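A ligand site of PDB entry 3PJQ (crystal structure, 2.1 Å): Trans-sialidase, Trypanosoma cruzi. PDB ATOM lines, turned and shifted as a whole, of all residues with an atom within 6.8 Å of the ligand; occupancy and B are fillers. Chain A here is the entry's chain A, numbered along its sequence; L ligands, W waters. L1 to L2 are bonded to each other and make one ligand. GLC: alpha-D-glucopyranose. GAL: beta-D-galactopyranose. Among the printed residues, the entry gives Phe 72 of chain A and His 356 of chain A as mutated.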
ATOM      1  N   ARG A  49       9.276 -29.828 -30.952  1.00  0.00           N
ATOM      2  CA  ARG A  49      10.244 -28.731 -30.697  1.00  0.00           C
ATOM      3  C   ARG A  49      10.995 -28.348 -31.973  1.00  0.00           C
ATOM      4  O   ARG A  49      10.883 -29.019 -32.976  1.00  0.00           O
ATOM      5  CB  ARG A  49      11.265 -29.206 -29.638  1.00  0.00           C
ATOM      6  CG  ARG A  49      10.632 -29.296 -28.219  1.00  0.00           C
ATOM      7  CD  ARG A  49      11.561 -28.925 -27.085  1.00  0.00           C
ATOM      8  NE  ARG A  49      12.094 -27.599 -27.321  1.00  0.00           N
ATOM      9  CZ  ARG A  49      13.330 -27.210 -27.019  1.00  0.00           C
ATOM     10  NH1 ARG A  49      13.708 -25.955 -27.337  1.00  0.00           N
ATOM     11  NH2 ARG A  49      14.181 -28.029 -26.421  1.00  0.00           N
ATOM     12  N   LEU A  50      11.760 -27.268 -31.930  1.00  0.00           N
ATOM     13  CA  LEU A  50      12.696 -26.883 -33.023  1.00  0.00           C
ATOM     14  C   LEU A  50      11.972 -26.568 -34.328  1.00  0.00           C
ATOM     15  O   LEU A  50      12.298 -27.118 -35.391  1.00  0.00           O
ATOM     16  CB  LEU A  50      13.830 -27.942 -33.212  1.00  0.00           C
ATOM     17  CG  LEU A  50      14.984 -27.971 -32.186  1.00  0.00           C
ATOM     18  CD1 LEU A  50      14.593 -27.554 -30.754  1.00  0.00           C
ATOM     19  CD2 LEU A  50      15.628 -29.363 -32.153  1.00  0.00           C
ATOM     20  N   ARG A  67       9.542 -35.388 -30.616  1.00  0.00           N
ATOM     21  CA  ARG A  67      10.143 -35.989 -29.458  1.00  0.00           C
ATOM     22  C   ARG A  67       9.118 -36.925 -28.821  1.00  0.00           C
ATOM     23  O   ARG A  67       8.292 -36.511 -28.009  1.00  0.00           O
ATOM     24  CB  ARG A  67      10.619 -34.907 -28.523  1.00  0.00           C
ATOM     25  CG  ARG A  67      11.344 -33.781 -29.193  1.00  0.00           C
ATOM     26  CD  ARG A  67      12.382 -33.290 -28.216  1.00  0.00           C
ATOM     27  NE  ARG A  67      13.215 -32.268 -28.823  1.00  0.00           N
ATOM     28  CZ  ARG A  67      14.127 -31.541 -28.180  1.00  0.00           C
ATOM     29  NH1 ARG A  67      14.355 -31.705 -26.878  1.00  0.00           N
ATOM     30  NH2 ARG A  67      14.774 -30.611 -28.842  1.00  0.00           N
ATOM     31  N   SER A  71      10.248 -34.655 -23.600  1.00  0.00           N
ATOM     32  CA  SER A  71      10.918 -33.511 -24.242  1.00  0.00           C
ATOM     33  C   SER A  71      12.453 -33.478 -23.989  1.00  0.00           C
ATOM     34  O   SER A  71      13.104 -32.579 -24.470  1.00  0.00           O
ATOM     35  CB  SER A  71      10.306 -32.177 -23.792  1.00  0.00           C
ATOM     36  OG  SER A  71      10.455 -32.058 -22.362  1.00  0.00           O
ATOM     37  N   PHE A  72      13.009 -34.422 -23.228  1.00  0.00           N
ATOM     38  CA  PHE A  72      14.479 -34.514 -22.974  1.00  0.00           C
ATOM     39  C   PHE A  72      15.178 -34.480 -24.336  1.00  0.00           C
ATOM     40  O   PHE A  72      14.802 -35.239 -25.221  1.00  0.00           O
ATOM     41  CB  PHE A  72      14.804 -35.797 -22.156  1.00  0.00           C
ATOM     42  CG  PHE A  72      16.243 -35.891 -21.674  1.00  0.00           C
ATOM     43  CD1 PHE A  72      16.882 -34.794 -21.084  1.00  0.00           C
ATOM     44  CD2 PHE A  72      16.959 -37.089 -21.814  1.00  0.00           C
ATOM     45  CE1 PHE A  72      18.241 -34.899 -20.644  1.00  0.00           C
ATOM     46  CE2 PHE A  72      18.308 -37.228 -21.327  1.00  0.00           C
ATOM     47  CZ  PHE A  72      18.941 -36.140 -20.745  1.00  0.00           C
ATOM     48  N   ASP A  73      16.103 -33.549 -24.522  1.00  0.00           N
ATOM     49  CA  ASP A  73      16.957 -33.485 -25.707  1.00  0.00           C
ATOM     50  C   ASP A  73      17.515 -34.864 -26.146  1.00  0.00           C
ATOM     51  O   ASP A  73      17.482 -35.204 -27.349  1.00  0.00           O
ATOM     52  CB  ASP A  73      18.161 -32.574 -25.431  1.00  0.00           C
ATOM     53  CG  ASP A  73      17.844 -31.089 -25.509  1.00  0.00           C
ATOM     54  OD1 ASP A  73      16.675 -30.684 -25.566  1.00  0.00           O
ATOM     55  OD2 ASP A  73      18.783 -30.295 -25.500  1.00  0.00           O
ATOM     56  N   TYR A 133      24.296 -34.549 -22.991  1.00  0.00           N
ATOM     57  CA  TYR A 133      24.157 -33.419 -23.955  1.00  0.00           C
ATOM     58  C   TYR A 133      25.415 -33.338 -24.817  1.00  0.00           C
ATOM     59  O   TYR A 133      26.555 -33.674 -24.331  1.00  0.00           O
ATOM     60  CB  TYR A 133      23.987 -32.162 -23.157  1.00  0.00           C
ATOM     61  CG  TYR A 133      22.634 -32.042 -22.443  1.00  0.00           C
ATOM     62  CD1 TYR A 133      22.545 -32.268 -21.053  1.00  0.00           C
ATOM     63  CD2 TYR A 133      21.445 -31.649 -23.149  1.00  0.00           C
ATOM     64  CE1 TYR A 133      21.322 -32.131 -20.348  1.00  0.00           C
ATOM     65  CE2 TYR A 133      20.188 -31.516 -22.459  1.00  0.00           C
ATOM     66  CZ  TYR A 133      20.159 -31.726 -21.066  1.00  0.00           C
ATOM     67  OH  TYR A 133      18.997 -31.609 -20.353  1.00  0.00           O
ATOM     68  N   THR A 135      27.486 -31.142 -26.208  1.00  0.00           N
ATOM     69  CA  THR A 135      28.628 -30.235 -25.886  1.00  0.00           C
ATOM     70  C   THR A 135      29.513 -30.852 -24.819  1.00  0.00           C
ATOM     71  O   THR A 135      30.618 -30.379 -24.586  1.00  0.00           O
ATOM     72  CB  THR A 135      28.084 -28.952 -25.324  1.00  0.00           C
ATOM     73  OG1 THR A 135      26.899 -29.288 -24.581  1.00  0.00           O
ATOM     74  CG2 THR A 135      27.663 -27.952 -26.464  1.00  0.00           C
ATOM     75  N   GLU A 244      24.137 -22.046 -31.873  1.00  0.00           N
ATOM     76  CA  GLU A 244      22.902 -21.866 -32.692  1.00  0.00           C
ATOM     77  C   GLU A 244      22.902 -20.650 -33.628  1.00  0.00           C
ATOM     78  O   GLU A 244      21.941 -19.907 -33.646  1.00  0.00           O
ATOM     79  CB  GLU A 244      21.626 -21.899 -31.821  1.00  0.00           C
ATOM     80  CG  GLU A 244      21.406 -23.253 -31.080  1.00  0.00           C
ATOM     81  CD  GLU A 244      20.201 -23.263 -30.086  1.00  0.00           C
ATOM     82  OE1 GLU A 244      19.939 -22.238 -29.399  1.00  0.00           O
ATOM     83  OE2 GLU A 244      19.542 -24.348 -29.954  1.00  0.00           O
ATOM     84  N   ARG A 259      23.746 -17.165 -30.702  1.00  0.00           N
ATOM     85  CA  ARG A 259      23.443 -17.342 -29.247  1.00  0.00           C
ATOM     86  C   ARG A 259      24.704 -17.411 -28.429  1.00  0.00           C
ATOM     87  O   ARG A 259      25.700 -18.075 -28.816  1.00  0.00           O
ATOM     88  CB  ARG A 259      22.696 -18.656 -29.061  1.00  0.00           C
ATOM     89  CG  ARG A 259      22.561 -19.181 -27.624  1.00  0.00           C
ATOM     90  CD  ARG A 259      21.741 -20.466 -27.607  1.00  0.00           C
ATOM     91  NE  ARG A 259      21.688 -20.923 -26.220  1.00  0.00           N
ATOM     92  CZ  ARG A 259      21.042 -22.016 -25.806  1.00  0.00           C
ATOM     93  NH1 ARG A 259      20.322 -22.751 -26.679  1.00  0.00           N
ATOM     94  NH2 ARG A 259      21.080 -22.333 -24.522  1.00  0.00           N
ATOM     95  N   TYR A 262      24.556 -16.660 -21.237  1.00  0.00           N
ATOM     96  CA  TYR A 262      24.979 -15.769 -20.149  1.00  0.00           C
ATOM     97  C   TYR A 262      25.618 -14.455 -20.661  1.00  0.00           C
ATOM     98  O   TYR A 262      26.224 -13.707 -19.889  1.00  0.00           O
ATOM     99  CB  TYR A 262      25.801 -16.509 -19.060  1.00  0.00           C
ATOM    100  CG  TYR A 262      25.229 -17.869 -18.738  1.00  0.00           C
ATOM    101  CD1 TYR A 262      25.712 -19.013 -19.381  1.00  0.00           C
ATOM    102  CD2 TYR A 262      24.192 -18.014 -17.834  1.00  0.00           C
ATOM    103  CE1 TYR A 262      25.193 -20.247 -19.139  1.00  0.00           C
ATOM    104  CE2 TYR A 262      23.674 -19.264 -17.573  1.00  0.00           C
ATOM    105  CZ  TYR A 262      24.182 -20.376 -18.238  1.00  0.00           C
ATOM    106  OH  TYR A 262      23.701 -21.629 -17.982  1.00  0.00           O
ATOM    107  N   ARG A 325      16.638 -19.306 -16.636  1.00  0.00           N
ATOM    108  CA  ARG A 325      17.020 -20.655 -17.117  1.00  0.00           C
ATOM    109  C   ARG A 325      16.575 -20.893 -18.564  1.00  0.00           C
ATOM    110  O   ARG A 325      16.689 -19.949 -19.361  1.00  0.00           O
ATOM    111  CB  ARG A 325      16.587 -21.727 -16.181  1.00  0.00           C
ATOM    112  CG  ARG A 325      17.496 -21.713 -14.992  1.00  0.00           C
ATOM    113  CD  ARG A 325      17.040 -22.734 -13.983  1.00  0.00           C
ATOM    114  NE  ARG A 325      17.433 -24.097 -14.334  1.00  0.00           N
ATOM    115  CZ  ARG A 325      18.578 -24.689 -13.956  1.00  0.00           C
ATOM    116  NH1 ARG A 325      19.496 -24.019 -13.254  1.00  0.00           N
ATOM    117  NH2 ARG A 325      18.823 -25.965 -14.303  1.00  0.00           N
ATOM    118  N   TRP A 326      16.028 -22.070 -18.882  1.00  0.00           N
ATOM    119  CA  TRP A 326      15.540 -22.370 -20.220  1.00  0.00           C
ATOM    120  C   TRP A 326      14.028 -22.180 -20.413  1.00  0.00           C
ATOM    121  O   TRP A 326      13.485 -22.424 -21.508  1.00  0.00           O
ATOM    122  CB  TRP A 326      15.962 -23.746 -20.704  1.00  0.00           C
ATOM    123  CG  TRP A 326      17.456 -23.850 -20.817  1.00  0.00           C
ATOM    124  CD1 TRP A 326      18.201 -23.660 -21.953  1.00  0.00           C
ATOM    125  CD2 TRP A 326      18.393 -24.114 -19.754  1.00  0.00           C
ATOM    126  NE1 TRP A 326      19.527 -23.837 -21.674  1.00  0.00           N
ATOM    127  CE2 TRP A 326      19.687 -24.096 -20.340  1.00  0.00           C
ATOM    128  CE3 TRP A 326      18.267 -24.362 -18.383  1.00  0.00           C
ATOM    129  CZ2 TRP A 326      20.855 -24.352 -19.598  1.00  0.00           C
ATOM    130  CZ3 TRP A 326      19.422 -24.595 -17.631  1.00  0.00           C
ATOM    131  CH2 TRP A 326      20.713 -24.598 -18.252  1.00  0.00           C
ATOM    132  N   LEU A 327      13.364 -21.680 -19.359  1.00  0.00           N
ATOM    133  CA  LEU A 327      11.939 -21.284 -19.430  1.00  0.00           C
ATOM    134  C   LEU A 327      11.621 -20.374 -20.669  1.00  0.00           C
ATOM    135  O   LEU A 327      10.800 -20.773 -21.530  1.00  0.00           O
ATOM    136  CB  LEU A 327      11.429 -20.728 -18.078  1.00  0.00           C
ATOM    137  CG  LEU A 327      11.444 -21.762 -16.955  1.00  0.00           C
ATOM    138  CD1 LEU A 327      11.003 -21.077 -15.649  1.00  0.00           C
ATOM    139  CD2 LEU A 327      10.633 -23.098 -17.235  1.00  0.00           C
ATOM    140  N   ARG A 328      12.292 -19.213 -20.798  1.00  0.00           N
ATOM    141  CA  ARG A 328      12.329 -18.503 -22.090  1.00  0.00           C
ATOM    142  C   ARG A 328      10.904 -18.049 -22.563  1.00  0.00           C
ATOM    143  O   ARG A 328      10.469 -18.282 -23.701  1.00  0.00           O
ATOM    144  CB  ARG A 328      13.130 -19.318 -23.138  1.00  0.00           C
ATOM    145  CG  ARG A 328      14.636 -19.497 -22.630  1.00  0.00           C
ATOM    146  CD  ARG A 328      15.553 -20.234 -23.583  1.00  0.00           C
ATOM    147  NE  ARG A 328      15.234 -21.659 -23.766  1.00  0.00           N
ATOM    148  CZ  ARG A 328      15.890 -22.468 -24.596  1.00  0.00           C
ATOM    149  NH1 ARG A 328      16.938 -21.982 -25.307  1.00  0.00           N
ATOM    150  NH2 ARG A 328      15.566 -23.769 -24.669  1.00  0.00           N
ATOM    151  N   HIS A 356      11.684 -21.403 -29.077  1.00  0.00           N
ATOM    152  CA  HIS A 356      12.022 -21.279 -30.504  1.00  0.00           C
ATOM    153  C   HIS A 356      10.895 -20.759 -31.323  1.00  0.00           C
ATOM    154  O   HIS A 356       9.733 -20.867 -30.897  1.00  0.00           O
ATOM    155  CB  HIS A 356      12.402 -22.593 -31.111  1.00  0.00           C
ATOM    156  CG  HIS A 356      13.601 -23.224 -30.485  1.00  0.00           C
ATOM    157  ND1 HIS A 356      14.541 -23.886 -31.235  1.00  0.00           N
ATOM    158  CD2 HIS A 356      14.037 -23.269 -29.202  1.00  0.00           C
ATOM    159  CE1 HIS A 356      15.497 -24.364 -30.440  1.00  0.00           C
ATOM    160  NE2 HIS A 356      15.204 -24.022 -29.190  1.00  0.00           N
ATOM    161  N   ASN A 373       5.496 -23.944 -24.092  1.00  0.00           N
ATOM    162  CA  ASN A 373       5.834 -25.010 -23.113  1.00  0.00           C
ATOM    163  C   ASN A 373       5.150 -24.893 -21.738  1.00  0.00           C
ATOM    164  O   ASN A 373       5.360 -23.914 -20.999  1.00  0.00           O
ATOM    165  CB  ASN A 373       7.368 -25.040 -22.998  1.00  0.00           C
ATOM    166  CG  ASN A 373       7.868 -25.558 -21.661  1.00  0.00           C
ATOM    167  OD1 ASN A 373       8.818 -25.014 -21.153  1.00  0.00           O
ATOM    168  ND2 ASN A 373       7.232 -26.562 -21.098  1.00  0.00           N
ATOM    169  N   GLU A 376       7.416 -28.628 -19.348  1.00  0.00           N
ATOM    170  CA  GLU A 376       8.265 -29.431 -20.216  1.00  0.00           C
ATOM    171  C   GLU A 376       7.488 -30.372 -21.151  1.00  0.00           C
ATOM    172  O   GLU A 376       7.926 -31.449 -21.522  1.00  0.00           O
ATOM    173  CB  GLU A 376       9.367 -30.160 -19.408  1.00  0.00           C
ATOM    174  CG  GLU A 376      10.292 -29.163 -18.629  1.00  0.00           C
ATOM    175  CD  GLU A 376      10.768 -27.973 -19.477  1.00  0.00           C
ATOM    176  OE1 GLU A 376      11.469 -28.205 -20.500  1.00  0.00           O
ATOM    177  OE2 GLU A 376      10.387 -26.807 -19.159  1.00  0.00           O
ATOM    178  N   TYR A 378       5.899 -29.659 -24.837  1.00  0.00           N
ATOM    179  CA  TYR A 378       5.897 -28.605 -25.845  1.00  0.00           C
ATOM    180  C   TYR A 378       4.967 -28.951 -26.957  1.00  0.00           C
ATOM    181  O   TYR A 378       4.964 -30.080 -27.430  1.00  0.00           O
ATOM    182  CB  TYR A 378       7.267 -28.397 -26.491  1.00  0.00           C
ATOM    183  CG  TYR A 378       8.379 -28.085 -25.523  1.00  0.00           C
ATOM    184  CD1 TYR A 378       8.688 -28.974 -24.451  1.00  0.00           C
ATOM    185  CD2 TYR A 378       9.118 -26.920 -25.655  1.00  0.00           C
ATOM    186  CE1 TYR A 378       9.725 -28.665 -23.537  1.00  0.00           C
ATOM    187  CE2 TYR A 378      10.171 -26.642 -24.770  1.00  0.00           C
ATOM    188  CZ  TYR A 378      10.464 -27.491 -23.728  1.00  0.00           C
ATOM    189  OH  TYR A 378      11.522 -27.167 -22.862  1.00  0.00           O
HETATM  190  C1  GLC L   1      21.142 -28.660 -16.828  1.00  0.00           C
HETATM  191  C2  GLC L   1      19.713 -28.059 -16.958  1.00  0.00           C
HETATM  192  C3  GLC L   1      19.124 -28.484 -18.301  1.00  0.00           C
HETATM  193  C4  GLC L   1      20.010 -27.996 -19.480  1.00  0.00           C
HETATM  194  C5  GLC L   1      21.495 -28.424 -19.275  1.00  0.00           C
HETATM  195  C6  GLC L   1      22.481 -27.771 -20.234  1.00  0.00           C
HETATM  196  O1  GLC L   1      21.167 -30.091 -16.943  1.00  0.00           O
HETATM  197  O2  GLC L   1      18.774 -28.392 -15.911  1.00  0.00           O
HETATM  198  O3  GLC L   1      17.766 -28.001 -18.345  1.00  0.00           O
HETATM  199  O4  GLC L   1      19.562 -28.516 -20.736  1.00  0.00           O
HETATM  200  O5  GLC L   1      21.939 -28.146 -17.923  1.00  0.00           O
HETATM  201  O6  GLC L   1      23.727 -28.476 -20.209  1.00  0.00           O
HETATM  202  C1  GAL L   2      18.579 -27.699 -21.365  1.00  0.00           C
HETATM  203  C2  GAL L   2      18.695 -27.952 -22.860  1.00  0.00           C
HETATM  204  C3  GAL L   2      17.527 -27.347 -23.668  1.00  0.00           C
HETATM  205  C4  GAL L   2      16.155 -27.795 -23.114  1.00  0.00           C
HETATM  206  C5  GAL L   2      16.135 -27.500 -21.590  1.00  0.00           C
HETATM  207  C6  GAL L   2      14.847 -27.945 -20.893  1.00  0.00           C
HETATM  208  O2  GAL L   2      19.877 -27.310 -23.308  1.00  0.00           O
HETATM  209  O3  GAL L   2      17.749 -27.654 -25.055  1.00  0.00           O
HETATM  210  O4  GAL L   2      15.885 -29.198 -23.366  1.00  0.00           O
HETATM  211  O5  GAL L   2      17.270 -28.099 -20.923  1.00  0.00           O
HETATM  212  O6  GAL L   2      14.798 -27.310 -19.634  1.00  0.00           O
HETATM  213  O   HOH W   1      16.223 -26.369 -16.562  1.00  0.00           O
HETATM  214  O   HOH W   2      22.030 -28.480 -23.154  1.00  0.00           O
HETATM  215  O   HOH W   3      23.897 -30.630 -17.108  1.00  0.00           O
HETATM  216  O   HOH W   4      20.194 -25.319 -24.801  1.00  0.00           O
HETATM  217  O   HOH W   5      16.497 -31.568 -22.628  1.00  0.00           O
HETATM  218  O   HOH W   6      23.428 -25.849 -17.662  1.00  0.00           O
HETATM  219  O   HOH W   7      13.477 -29.790 -24.152  1.00  0.00           O
HETATM  220  O   HOH W   8      17.355 -31.018 -16.833  1.00  0.00           O
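NH2 of Arg 325 is in hydrogen-bond range of O2 of GLC L1.
An oxygen (O4) of GAL L2 sits at hydrogen-bond distance from the side-chain carboxylate (OD1) of Asp 73, at 2.8 Å.
The side-chain hydroxyl (OH) of Tyr 133 is in hydrogen-bond range of an oxygen (O4) of GLC L1 (3.2 Å).
NE of Arg 328 is in hydrogen-bond range of O of Trp 326 (3.0 Å).
The side-chain carboxylate (OD1) of Asp 73 is in salt-bridge range of the guanidinium group (NH2) of Arg 49 (3.7 Å).
OE1 of Glu 376 is in hydrogen-bond range of OH of Tyr 378 (2.6 Å).
The side-chain hydroxyl of Ser 71 lies within hydrogen-bond range of the backbone carbonyl oxygen of Glu 376 (2.7 Å).
The backbone NH of Glu 376 lies close to the side-chain amide nitrogen of Asn 373, 2.7 Å away.
A ring nitrogen (NE2) of His 356 is in hydrogen-bond range of the guanidinium group (NH1) of Arg 49 (3.1 Å).
The side-chain carboxylate (OD1) of Asp 73 lies within salt-bridge range of the guanidinium group (NH1) of Arg 67, 2.9 Å away.
Arg 49 touches the ligand.
Trp 326 touches the ligand.
Glu 376 touches the ligand.
Tyr 378 touches the ligand.
Hydrophobic or aromatic side chains that line the ligand: Tyr 133 and Trp 326.
Seven residues have an atom within 4 Å of the ligand: Arg 49, Asp 73, Tyr 133, Arg 325, Trp 326, Glu 376 and Tyr 378.
Along chain A the residues within 4 Å of the ligand span positions 49 to 378.
Water W4 bridges O2 of GAL L2 (2.5 Å) and NH2 of Arg 259 (3.1 Å).
Water W5 lies within hydrogen-bond range of O4 of GAL L2 (2.6 Å), N of Asp 73 (2.8 Å) and OH of Tyr 133 (3.4 Å).
Water W7 lies within hydrogen-bond range of O4 of GAL L2 (2.6 Å), O of Ser 71 (2.8 Å), NH2 of Arg 49 (3.0 Å) and NH1 of Arg 67 (3.4 Å).
Water W1 bridges an oxygen (O3) of GLC L1 (2.9 Å) and the guanidinium group (NE) of Arg 325 (3.4 Å).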
